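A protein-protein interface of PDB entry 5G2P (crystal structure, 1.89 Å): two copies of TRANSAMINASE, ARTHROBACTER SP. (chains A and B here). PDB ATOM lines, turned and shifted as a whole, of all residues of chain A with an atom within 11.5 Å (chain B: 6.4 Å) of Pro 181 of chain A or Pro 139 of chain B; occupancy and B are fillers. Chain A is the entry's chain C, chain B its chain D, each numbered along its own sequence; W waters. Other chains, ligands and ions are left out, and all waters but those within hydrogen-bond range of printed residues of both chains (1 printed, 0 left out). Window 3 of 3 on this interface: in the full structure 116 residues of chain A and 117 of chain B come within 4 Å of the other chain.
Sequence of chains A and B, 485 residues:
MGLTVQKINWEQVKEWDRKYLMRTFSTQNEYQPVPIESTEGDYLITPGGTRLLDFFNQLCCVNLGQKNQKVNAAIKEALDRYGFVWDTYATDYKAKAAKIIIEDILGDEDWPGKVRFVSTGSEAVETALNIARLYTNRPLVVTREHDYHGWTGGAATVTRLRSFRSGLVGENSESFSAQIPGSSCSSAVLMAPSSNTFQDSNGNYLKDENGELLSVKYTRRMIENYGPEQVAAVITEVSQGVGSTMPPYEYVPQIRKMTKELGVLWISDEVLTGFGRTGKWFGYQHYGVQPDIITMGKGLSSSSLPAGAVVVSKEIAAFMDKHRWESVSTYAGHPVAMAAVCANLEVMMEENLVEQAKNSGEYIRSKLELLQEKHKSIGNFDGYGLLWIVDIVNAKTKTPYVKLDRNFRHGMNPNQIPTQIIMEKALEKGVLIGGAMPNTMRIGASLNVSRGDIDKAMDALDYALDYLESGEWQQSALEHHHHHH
The backbone NH (N) of Arg 138 of chain B is in hydrogen-bond range of the backbone carbonyl oxygen (O) of Arg 133 of chain B (3.3 Å).
The guanidinium group of Arg 133 of chain B sits at hydrogen-bond distance from the backbone carbonyl oxygen of Pro 139 of chain B.
The backbone carbonyl oxygen (O) of Ala 188 of chain B is in hydrogen-bond range of the guanidinium group (NH2) of Arg 133 of chain B, 3.1 Å away.
N of Arg 138 of chain B sits close to OG1 of Thr 136 of chain B (3.3 Å).
The backbone carbonyl oxygen of Val 231 of chain B is in hydrogen-bond range of the guanidinium group of Arg 138 of chain B (2.8 Å).
Among the printed residues, merely in contact across the chains: Ser 166 of chain A with Leu 134 of chain B, Ile 180 of chain A with Asn 130 of chain B, Ile 180 of chain A with Arg 133 of chain B, Ile 180 of chain A with Leu 134 of chain B, Pro 181 of chain A with Arg 133 of chain B, Pro 181 of chain A with Asn 137 of chain B, Pro 181 of chain A with Arg 138 of chain B and Pro 181 of chain A with Pro 139 of chain B.
Of the printed residues of chain B, Ser 166 of chain A touches Leu 134.
Of the printed residues of chain B, Ile 180 of chain A touches Asn 130, Arg 133 and Leu 134.
Of the printed residues of chain A, Asn 130 of chain B touches Ile 180 (3.5 Å).
Arg 133 of chain B touches two residues of chain A.
Of chain A, only Ser 166 (3.5 Å) and Ile 180 (3.9 Å) come within 4 Å of Leu 134 of chain B.
Of chain A, only Pro 181 (3.6 Å) comes within 4 Å of Asn 137 of chain B.
Of the printed residues of chain A, Arg 138 of chain B touches Pro 181.
Pro 139 of chain B touches just one residue of chain A: Pro 181 (3.7 Å).
No residue of chain A comes within 4 Å of Leu 140 of chain B.
Val 141 of chain B touches none of the printed residues of chain A.
Ala 188 of chain B touches none of the printed residues of chain A.
No residue of chain A comes within 4 Å of Gln 230 of chain B.
No residue of chain A comes within 4 Å of Val 231 of chain B.
The nearest residue of chain B that does not touch Pro 181 of chain A is Leu 134 of chain B (4.2 Å).
Of the 16 printed residues of chain B, 6 touch a printed residue of chain A.
Printed residues of chain A that touch a printed residue of chain B: Ser 166, Ile 180 and Pro 181.
Among the printed residues, 8 pairs touch across the chains.
Among the printed residues, no Asp or Glu carboxylate lies within 4 Å of a Lys or Arg side-chain nitrogen of the other chain.
1 position is printed for both chains.
Water W1 bridges the side-chain amide nitrogen of Asn 130 of chain B (2.9 Å) and the backbone NH of Gly 153 of chain A (3.4 Å).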
ATOM      1  N   GLY A 153      23.531  27.358   5.948  1.00  0.00           N
ATOM      2  CA  GLY A 153      22.162  27.359   5.379  1.00  0.00           C
ATOM      3  C   GLY A 153      21.838  26.461   4.179  1.00  0.00           C
ATOM      4  O   GLY A 153      20.947  25.615   4.269  1.00  0.00           O
ATOM      5  N   ALA A 156      23.046  22.818   4.832  1.00  0.00           N
ATOM      6  CA  ALA A 156      22.153  22.147   5.770  1.00  0.00           C
ATOM      7  C   ALA A 156      20.842  21.630   5.140  1.00  0.00           C
ATOM      8  O   ALA A 156      20.302  20.601   5.610  1.00  0.00           O
ATOM      9  CB  ALA A 156      21.847  23.021   6.997  1.00  0.00           C
ATOM     10  N   THR A 157      20.341  22.320   4.106  1.00  0.00           N
ATOM     11  CA  THR A 157      19.080  21.919   3.462  1.00  0.00           C
ATOM     12  C   THR A 157      19.192  20.518   2.874  1.00  0.00           C
ATOM     13  O   THR A 157      18.207  19.804   2.808  1.00  0.00           O
ATOM     14  CB  THR A 157      18.570  22.886   2.363  1.00  0.00           C
ATOM     15  OG1 THR A 157      19.521  22.961   1.285  1.00  0.00           O
ATOM     16  CG2 THR A 157      18.244  24.253   2.919  1.00  0.00           C
ATOM     17  N   ARG A 165      21.757  18.966  12.722  1.00  0.00           N
ATOM     18  CA  ARG A 165      21.178  20.141  12.036  1.00  0.00           C
ATOM     19  C   ARG A 165      21.187  21.414  12.897  1.00  0.00           C
ATOM     20  O   ARG A 165      20.392  22.335  12.679  1.00  0.00           O
ATOM     21  CB  ARG A 165      19.742  19.824  11.525  1.00  0.00           C
ATOM     22  CG  ARG A 165      19.692  18.923  10.290  1.00  0.00           C
ATOM     23  CD  ARG A 165      20.098  19.658   8.998  1.00  0.00           C
ATOM     24  NE  ARG A 165      19.233  20.829   8.749  1.00  0.00           N
ATOM     25  CZ  ARG A 165      18.193  20.874   7.919  1.00  0.00           C
ATOM     26  NH1 ARG A 165      17.872  19.855   7.135  1.00  0.00           N
ATOM     27  NH2 ARG A 165      17.503  22.001   7.838  1.00  0.00           N
ATOM     28  N   SER A 166      22.101  21.464  13.869  1.00  0.00           N
ATOM     29  CA  SER A 166      22.369  22.676  14.664  1.00  0.00           C
ATOM     30  C   SER A 166      21.217  23.084  15.557  1.00  0.00           C
ATOM     31  O   SER A 166      21.110  24.262  15.949  1.00  0.00           O
ATOM     32  CB  SER A 166      22.836  23.864  13.808  1.00  0.00           C
ATOM     33  OG  SER A 166      23.943  23.503  13.009  1.00  0.00           O
ATOM     34  N   GLY A 167      20.377  22.113  15.907  1.00  0.00           N
ATOM     35  CA  GLY A 167      19.302  22.335  16.869  1.00  0.00           C
ATOM     36  C   GLY A 167      19.753  22.022  18.276  1.00  0.00           C
ATOM     37  O   GLY A 167      20.944  21.772  18.506  1.00  0.00           O
ATOM     38  N   LEU A 168      18.788  21.996  19.208  1.00  0.00           N
ATOM     39  CA  LEU A 168      19.059  21.890  20.636  1.00  0.00           C
ATOM     40  C   LEU A 168      18.324  20.718  21.246  1.00  0.00           C
ATOM     41  O   LEU A 168      17.178  20.455  20.888  1.00  0.00           O
ATOM     42  CB  LEU A 168      18.619  23.152  21.365  1.00  0.00           C
ATOM     43  CG  LEU A 168      19.321  24.462  21.001  1.00  0.00           C
ATOM     44  CD1 LEU A 168      18.663  25.605  21.763  1.00  0.00           C
ATOM     45  CD2 LEU A 168      20.838  24.397  21.251  1.00  0.00           C
ATOM     46  N   VAL A 169      19.008  19.987  22.127  1.00  0.00           N
ATOM     47  CA  VAL A 169      18.372  18.901  22.908  1.00  0.00           C
ATOM     48  C   VAL A 169      18.741  19.081  24.379  1.00  0.00           C
ATOM     49  O   VAL A 169      19.658  19.847  24.706  1.00  0.00           O
ATOM     50  CB  VAL A 169      18.747  17.486  22.397  1.00  0.00           C
ATOM     51  CG1 VAL A 169      18.195  17.248  20.990  1.00  0.00           C
ATOM     52  CG2 VAL A 169      20.253  17.268  22.411  1.00  0.00           C
ATOM     53  N   PHE A 176      13.431  19.139  26.186  1.00  0.00           N
ATOM     54  CA  PHE A 176      13.929  20.470  25.887  1.00  0.00           C
ATOM     55  C   PHE A 176      14.500  20.568  24.477  1.00  0.00           C
ATOM     56  O   PHE A 176      15.486  21.291  24.251  1.00  0.00           O
ATOM     57  CB  PHE A 176      15.001  20.869  26.910  1.00  0.00           C
ATOM     58  CG  PHE A 176      14.519  20.846  28.328  1.00  0.00           C
ATOM     59  CD1 PHE A 176      13.832  21.937  28.859  1.00  0.00           C
ATOM     60  CD2 PHE A 176      14.731  19.726  29.130  1.00  0.00           C
ATOM     61  CE1 PHE A 176      13.363  21.912  30.166  1.00  0.00           C
ATOM     62  CE2 PHE A 176      14.263  19.697  30.437  1.00  0.00           C
ATOM     63  CZ  PHE A 176      13.584  20.789  30.956  1.00  0.00           C
ATOM     64  N   SER A 177      13.879  19.873  23.524  1.00  0.00           N
ATOM     65  CA  SER A 177      14.436  19.810  22.184  1.00  0.00           C
ATOM     66  C   SER A 177      13.763  20.771  21.177  1.00  0.00           C
ATOM     67  O   SER A 177      12.572  21.071  21.297  1.00  0.00           O
ATOM     68  CB  SER A 177      14.443  18.379  21.687  1.00  0.00           C
ATOM     69  OG  SER A 177      13.242  18.159  21.006  1.00  0.00           O
ATOM     70  N   ALA A 178      14.558  21.287  20.229  1.00  0.00           N
ATOM     71  CA  ALA A 178      14.080  22.218  19.200  1.00  0.00           C
ATOM     72  C   ALA A 178      14.945  22.118  17.953  1.00  0.00           C
ATOM     73  O   ALA A 178      16.165  21.886  18.037  1.00  0.00           O
ATOM     74  CB  ALA A 178      14.064  23.663  19.707  1.00  0.00           C
ATOM     75  N   GLN A 179      14.324  22.258  16.794  1.00  0.00           N
ATOM     76  CA  GLN A 179      15.117  22.483  15.593  1.00  0.00           C
ATOM     77  C   GLN A 179      15.040  23.955  15.325  1.00  0.00           C
ATOM     78  O   GLN A 179      14.207  24.641  15.890  1.00  0.00           O
ATOM     79  CB  GLN A 179      14.657  21.628  14.408  1.00  0.00           C
ATOM     80  CG  GLN A 179      14.746  20.108  14.640  1.00  0.00           C
ATOM     81  CD  GLN A 179      16.161  19.519  14.608  1.00  0.00           C
ATOM     82  OE1 GLN A 179      17.165  20.241  14.594  1.00  0.00           O
ATOM     83  NE2 GLN A 179      16.240  18.186  14.622  1.00  0.00           N
ATOM     84  N   ILE A 180      15.929  24.474  14.492  1.00  0.00           N
ATOM     85  CA  ILE A 180      15.935  25.899  14.228  1.00  0.00           C
ATOM     86  C   ILE A 180      14.612  26.344  13.557  1.00  0.00           C
ATOM     87  O   ILE A 180      14.251  25.788  12.510  1.00  0.00           O
ATOM     88  CB  ILE A 180      17.159  26.299  13.374  1.00  0.00           C
ATOM     89  CG1 ILE A 180      18.463  25.864  14.079  1.00  0.00           C
ATOM     90  CG2 ILE A 180      17.128  27.803  13.082  1.00  0.00           C
ATOM     91  CD1 ILE A 180      19.714  26.009  13.223  1.00  0.00           C
ATOM     92  N   PRO A 181      13.883  27.325  14.163  1.00  0.00           N
ATOM     93  CA  PRO A 181      12.685  27.896  13.515  1.00  0.00           C
ATOM     94  C   PRO A 181      12.971  28.341  12.074  1.00  0.00           C
ATOM     95  O   PRO A 181      14.026  28.930  11.804  1.00  0.00           O
ATOM     96  CB  PRO A 181      12.362  29.128  14.377  1.00  0.00           C
ATOM     97  CG  PRO A 181      12.900  28.788  15.719  1.00  0.00           C
ATOM     98  CD  PRO A 181      14.133  27.940  15.484  1.00  0.00           C
ATOM     99  N   GLY A 182      12.049  28.019  11.167  1.00  0.00           N
ATOM    100  CA  GLY A 182      12.187  28.336   9.752  1.00  0.00           C
ATOM    101  C   GLY A 182      12.786  27.187   8.963  1.00  0.00           C
ATOM    102  O   GLY A 182      12.769  27.214   7.739  1.00  0.00           O
ATOM    103  N   SER A 183      13.315  26.189   9.674  1.00  0.00           N
ATOM    104  CA  SER A 183      13.878  24.947   9.119  1.00  0.00           C
ATOM    105  C   SER A 183      15.297  24.710   9.601  1.00  0.00           C
ATOM    106  O   SER A 183      15.508  24.116  10.663  1.00  0.00           O
ATOM    107  CB  SER A 183      13.822  24.909   7.593  1.00  0.00           C
ATOM    108  OG  SER A 183      12.480  24.813   7.161  1.00  0.00           O
ATOM    109  N   SER A 187      12.272  25.100   1.194  1.00  0.00           N
ATOM    110  CA  SER A 187      13.525  24.601   0.625  1.00  0.00           C
ATOM    111  C   SER A 187      13.294  24.063  -0.788  1.00  0.00           C
ATOM    112  O   SER A 187      12.228  23.531  -1.108  1.00  0.00           O
ATOM    113  CB  SER A 187      14.113  23.486   1.495  1.00  0.00           C
ATOM    114  OG  SER A 187      13.469  22.239   1.223  1.00  0.00           O
ATOM    115  N   ARG A 409      18.513  11.615  18.387  1.00  0.00           N
ATOM    116  CA  ARG A 409      19.143  12.904  18.680  1.00  0.00           C
ATOM    117  C   ARG A 409      19.966  12.791  19.969  1.00  0.00           C
ATOM    118  O   ARG A 409      19.902  11.775  20.651  1.00  0.00           O
ATOM    119  CB  ARG A 409      18.137  14.058  18.705  1.00  0.00           C
ATOM    120  CG  ARG A 409      17.560  14.393  17.346  1.00  0.00           C
ATOM    121  CD  ARG A 409      16.606  15.559  17.444  1.00  0.00           C
ATOM    122  NE  ARG A 409      17.327  16.827  17.559  1.00  0.00           N
ATOM    123  CZ  ARG A 409      16.741  17.988  17.820  1.00  0.00           C
ATOM    124  NH1 ARG A 409      15.415  18.036  18.005  1.00  0.00           N
ATOM    125  NH2 ARG A 409      17.464  19.100  17.869  1.00  0.00           N
ATOM    126  N   ASN B 130      21.234  31.349  13.309  1.00  0.00           N
ATOM    127  CA  ASN B 130      20.820  30.113  14.003  1.00  0.00           C
ATOM    128  C   ASN B 130      20.551  30.378  15.484  1.00  0.00           C
ATOM    129  O   ASN B 130      19.506  29.955  16.020  1.00  0.00           O
ATOM    130  CB  ASN B 130      21.865  29.006  13.827  1.00  0.00           C
ATOM    131  CG  ASN B 130      21.975  28.543  12.383  1.00  0.00           C
ATOM    132  OD1 ASN B 130      21.155  28.917  11.541  1.00  0.00           O
ATOM    133  ND2 ASN B 130      22.974  27.719  12.092  1.00  0.00           N
ATOM    134  N   ARG B 133      17.420  32.722  16.167  1.00  0.00           N
ATOM    135  CA  ARG B 133      16.166  32.013  15.938  1.00  0.00           C
ATOM    136  C   ARG B 133      15.932  30.997  17.066  1.00  0.00           C
ATOM    137  O   ARG B 133      14.812  30.863  17.533  1.00  0.00           O
ATOM    138  CB  ARG B 133      16.162  31.308  14.562  1.00  0.00           C
ATOM    139  CG  ARG B 133      16.059  32.276  13.401  1.00  0.00           C
ATOM    140  CD  ARG B 133      16.300  31.633  12.052  1.00  0.00           C
ATOM    141  NE  ARG B 133      15.735  32.519  11.033  1.00  0.00           N
ATOM    142  CZ  ARG B 133      16.340  32.841   9.890  1.00  0.00           C
ATOM    143  NH1 ARG B 133      17.550  32.360   9.646  1.00  0.00           N
ATOM    144  NH2 ARG B 133      15.744  33.675   9.015  1.00  0.00           N
ATOM    145  N   LEU B 134      16.979  30.272  17.471  1.00  0.00           N
ATOM    146  CA  LEU B 134      16.831  29.296  18.542  1.00  0.00           C
ATOM    147  C   LEU B 134      16.482  29.985  19.866  1.00  0.00           C
ATOM    148  O   LEU B 134      15.541  29.558  20.564  1.00  0.00           O
ATOM    149  CB  LEU B 134      18.100  28.431  18.710  1.00  0.00           C
ATOM    150  CG  LEU B 134      18.381  27.357  17.663  1.00  0.00           C
ATOM    151  CD1 LEU B 134      19.818  26.877  17.807  1.00  0.00           C
ATOM    152  CD2 LEU B 134      17.396  26.206  17.840  1.00  0.00           C
ATOM    153  N   THR B 136      15.117  32.954  20.533  1.00  0.00           N
ATOM    154  CA  THR B 136      13.764  33.515  20.559  1.00  0.00           C
ATOM    155  C   THR B 136      12.655  32.498  20.251  1.00  0.00           C
ATOM    156  O   THR B 136      11.482  32.773  20.536  1.00  0.00           O
ATOM    157  CB  THR B 136      13.614  34.689  19.580  1.00  0.00           C
ATOM    158  OG1 THR B 136      13.859  34.236  18.236  1.00  0.00           O
ATOM    159  CG2 THR B 136      14.574  35.844  19.954  1.00  0.00           C
ATOM    160  N   ASN B 137      13.015  31.353  19.660  1.00  0.00           N
ATOM    161  CA  ASN B 137      12.047  30.424  19.057  1.00  0.00           C
ATOM    162  C   ASN B 137      11.162  31.055  17.965  1.00  0.00           C
ATOM    163  O   ASN B 137       9.985  30.717  17.829  1.00  0.00           O
ATOM    164  CB  ASN B 137      11.195  29.679  20.116  1.00  0.00           C
ATOM    165  CG  ASN B 137      10.627  28.364  19.586  1.00  0.00           C
ATOM    166  OD1 ASN B 137      11.234  27.712  18.725  1.00  0.00           O
ATOM    167  ND2 ASN B 137       9.448  27.980  20.075  1.00  0.00           N
ATOM    168  N   ARG B 138      11.739  31.968  17.191  1.00  0.00           N
ATOM    169  CA  ARG B 138      10.992  32.691  16.159  1.00  0.00           C
ATOM    170  C   ARG B 138      11.716  32.562  14.819  1.00  0.00           C
ATOM    171  O   ARG B 138      12.958  32.527  14.806  1.00  0.00           O
ATOM    172  CB  ARG B 138      10.843  34.171  16.533  1.00  0.00           C
ATOM    173  CG  ARG B 138      10.168  34.433  17.873  1.00  0.00           C
ATOM    174  CD  ARG B 138      10.247  35.897  18.202  1.00  0.00           C
ATOM    175  NE  ARG B 138       9.926  36.184  19.601  1.00  0.00           N
ATOM    176  CZ  ARG B 138      10.225  37.346  20.176  1.00  0.00           C
ATOM    177  NH1 ARG B 138      10.836  38.302  19.472  1.00  0.00           N
ATOM    178  NH2 ARG B 138       9.915  37.565  21.454  1.00  0.00           N
ATOM    179  N   PRO B 139      10.956  32.489  13.700  1.00  0.00           N
ATOM    180  CA  PRO B 139      11.512  32.263  12.356  1.00  0.00           C
ATOM    181  C   PRO B 139      12.059  33.493  11.619  1.00  0.00           C
ATOM    182  O   PRO B 139      12.987  33.346  10.832  1.00  0.00           O
ATOM    183  CB  PRO B 139      10.313  31.737  11.561  1.00  0.00           C
ATOM    184  CG  PRO B 139       9.117  32.362  12.240  1.00  0.00           C
ATOM    185  CD  PRO B 139       9.478  32.495  13.697  1.00  0.00           C
ATOM    186  N   LEU B 140      11.467  34.675  11.809  1.00  0.00           N
ATOM    187  CA  LEU B 140      11.792  35.782  10.891  1.00  0.00           C
ATOM    188  C   LEU B 140      13.003  36.577  11.330  1.00  0.00           C
ATOM    189  O   LEU B 140      13.184  36.829  12.539  1.00  0.00           O
ATOM    190  CB  LEU B 140      10.587  36.715  10.624  1.00  0.00           C
ATOM    191  CG  LEU B 140       9.310  36.088  10.005  1.00  0.00           C
ATOM    192  CD1 LEU B 140       8.193  37.127   9.994  1.00  0.00           C
ATOM    193  CD2 LEU B 140       9.501  35.493   8.611  1.00  0.00           C
ATOM    194  N   VAL B 141      13.807  36.990  10.333  1.00  0.00           N
ATOM    195  CA  VAL B 141      14.912  37.917  10.537  1.00  0.00           C
ATOM    196  C   VAL B 141      14.754  39.101   9.574  1.00  0.00           C
ATOM    197  O   VAL B 141      14.480  38.932   8.382  1.00  0.00           O
ATOM    198  CB  VAL B 141      16.294  37.235  10.405  1.00  0.00           C
ATOM    199  CG1 VAL B 141      17.426  38.281  10.458  1.00  0.00           C
ATOM    200  CG2 VAL B 141      16.497  36.201  11.510  1.00  0.00           C
ATOM    201  N   SER B 187      12.827  34.359   2.327  1.00  0.00           N
ATOM    202  CA  SER B 187      12.234  33.121   2.812  1.00  0.00           C
ATOM    203  C   SER B 187      12.694  32.992   4.264  1.00  0.00           C
ATOM    204  O   SER B 187      13.838  32.622   4.553  1.00  0.00           O
ATOM    205  CB  SER B 187      12.675  31.936   1.963  1.00  0.00           C
ATOM    206  OG  SER B 187      11.556  31.222   1.463  1.00  0.00           O
ATOM    207  N   ALA B 188      11.787  33.360   5.158  1.00  0.00           N
ATOM    208  CA  ALA B 188      12.059  33.629   6.583  1.00  0.00           C
ATOM    209  C   ALA B 188      12.789  34.970   6.841  1.00  0.00           C
ATOM    210  O   ALA B 188      13.261  35.213   7.944  1.00  0.00           O
ATOM    211  CB  ALA B 188      12.767  32.465   7.257  1.00  0.00           C
ATOM    212  N   VAL B 189      12.871  35.828   5.822  1.00  0.00           N
ATOM    213  CA  VAL B 189      13.534  37.137   5.950  1.00  0.00           C
ATOM    214  C   VAL B 189      12.594  38.278   5.538  1.00  0.00           C
ATOM    215  O   VAL B 189      11.821  38.125   4.625  1.00  0.00           O
ATOM    216  CB  VAL B 189      14.832  37.184   5.115  1.00  0.00           C
ATOM    217  CG1 VAL B 189      15.429  38.601   5.067  1.00  0.00           C
ATOM    218  CG2 VAL B 189      15.845  36.184   5.659  1.00  0.00           C
ATOM    219  N   GLU B 229       6.016  38.603  17.829  1.00  0.00           N
ATOM    220  CA  GLU B 229       6.173  37.214  18.239  1.00  0.00           C
ATOM    221  C   GLU B 229       6.684  36.337  17.081  1.00  0.00           C
ATOM    222  O   GLU B 229       7.131  35.219  17.308  1.00  0.00           O
ATOM    223  CB  GLU B 229       4.879  36.679  18.905  1.00  0.00           C
ATOM    224  CG  GLU B 229       3.808  36.042  17.994  1.00  0.00           C
ATOM    225  CD  GLU B 229       3.072  37.021  17.085  1.00  0.00           C
ATOM    226  OE1 GLU B 229       3.212  38.263  17.252  1.00  0.00           O
ATOM    227  OE2 GLU B 229       2.344  36.527  16.181  1.00  0.00           O
ATOM    228  N   GLN B 230       6.661  36.861  15.853  1.00  0.00           N
ATOM    229  CA  GLN B 230       7.179  36.115  14.695  1.00  0.00           C
ATOM    230  C   GLN B 230       8.642  36.448  14.376  1.00  0.00           C
ATOM    231  O   GLN B 230       9.273  35.755  13.566  1.00  0.00           O
ATOM    232  CB  GLN B 230       6.329  36.394  13.432  1.00  0.00           C
ATOM    233  CG  GLN B 230       4.848  36.009  13.509  1.00  0.00           C
ATOM    234  CD  GLN B 230       4.632  34.574  13.941  1.00  0.00           C
ATOM    235  OE1 GLN B 230       5.374  33.686  13.535  1.00  0.00           O
ATOM    236  NE2 GLN B 230       3.623  34.340  14.795  1.00  0.00           N
ATOM    237  N   VAL B 231       9.155  37.527  14.971  1.00  0.00           N
ATOM    238  CA  VAL B 231      10.442  38.127  14.561  1.00  0.00           C
ATOM    239  C   VAL B 231      11.568  37.903  15.588  1.00  0.00           C
ATOM    240  O   VAL B 231      11.552  38.432  16.718  1.00  0.00           O
ATOM    241  CB  VAL B 231      10.268  39.639  14.221  1.00  0.00           C
ATOM    242  CG1 VAL B 231      11.573  40.258  13.718  1.00  0.00           C
ATOM    243  CG2 VAL B 231       9.143  39.835  13.193  1.00  0.00           C
ATOM    244  N   ALA B 232      12.557  37.123  15.176  1.00  0.00           N
ATOM    245  CA  ALA B 232      13.711  36.805  16.020  1.00  0.00           C
ATOM    246  C   ALA B 232      14.660  37.996  16.231  1.00  0.00           C
ATOM    247  O   ALA B 232      15.085  38.279  17.366  1.00  0.00           O
ATOM    248  CB  ALA B 232      14.475  35.627  15.412  1.00  0.00           C
HETATM  249  O   HOH W   1      23.029  26.932   9.282  1.00  0.00           O
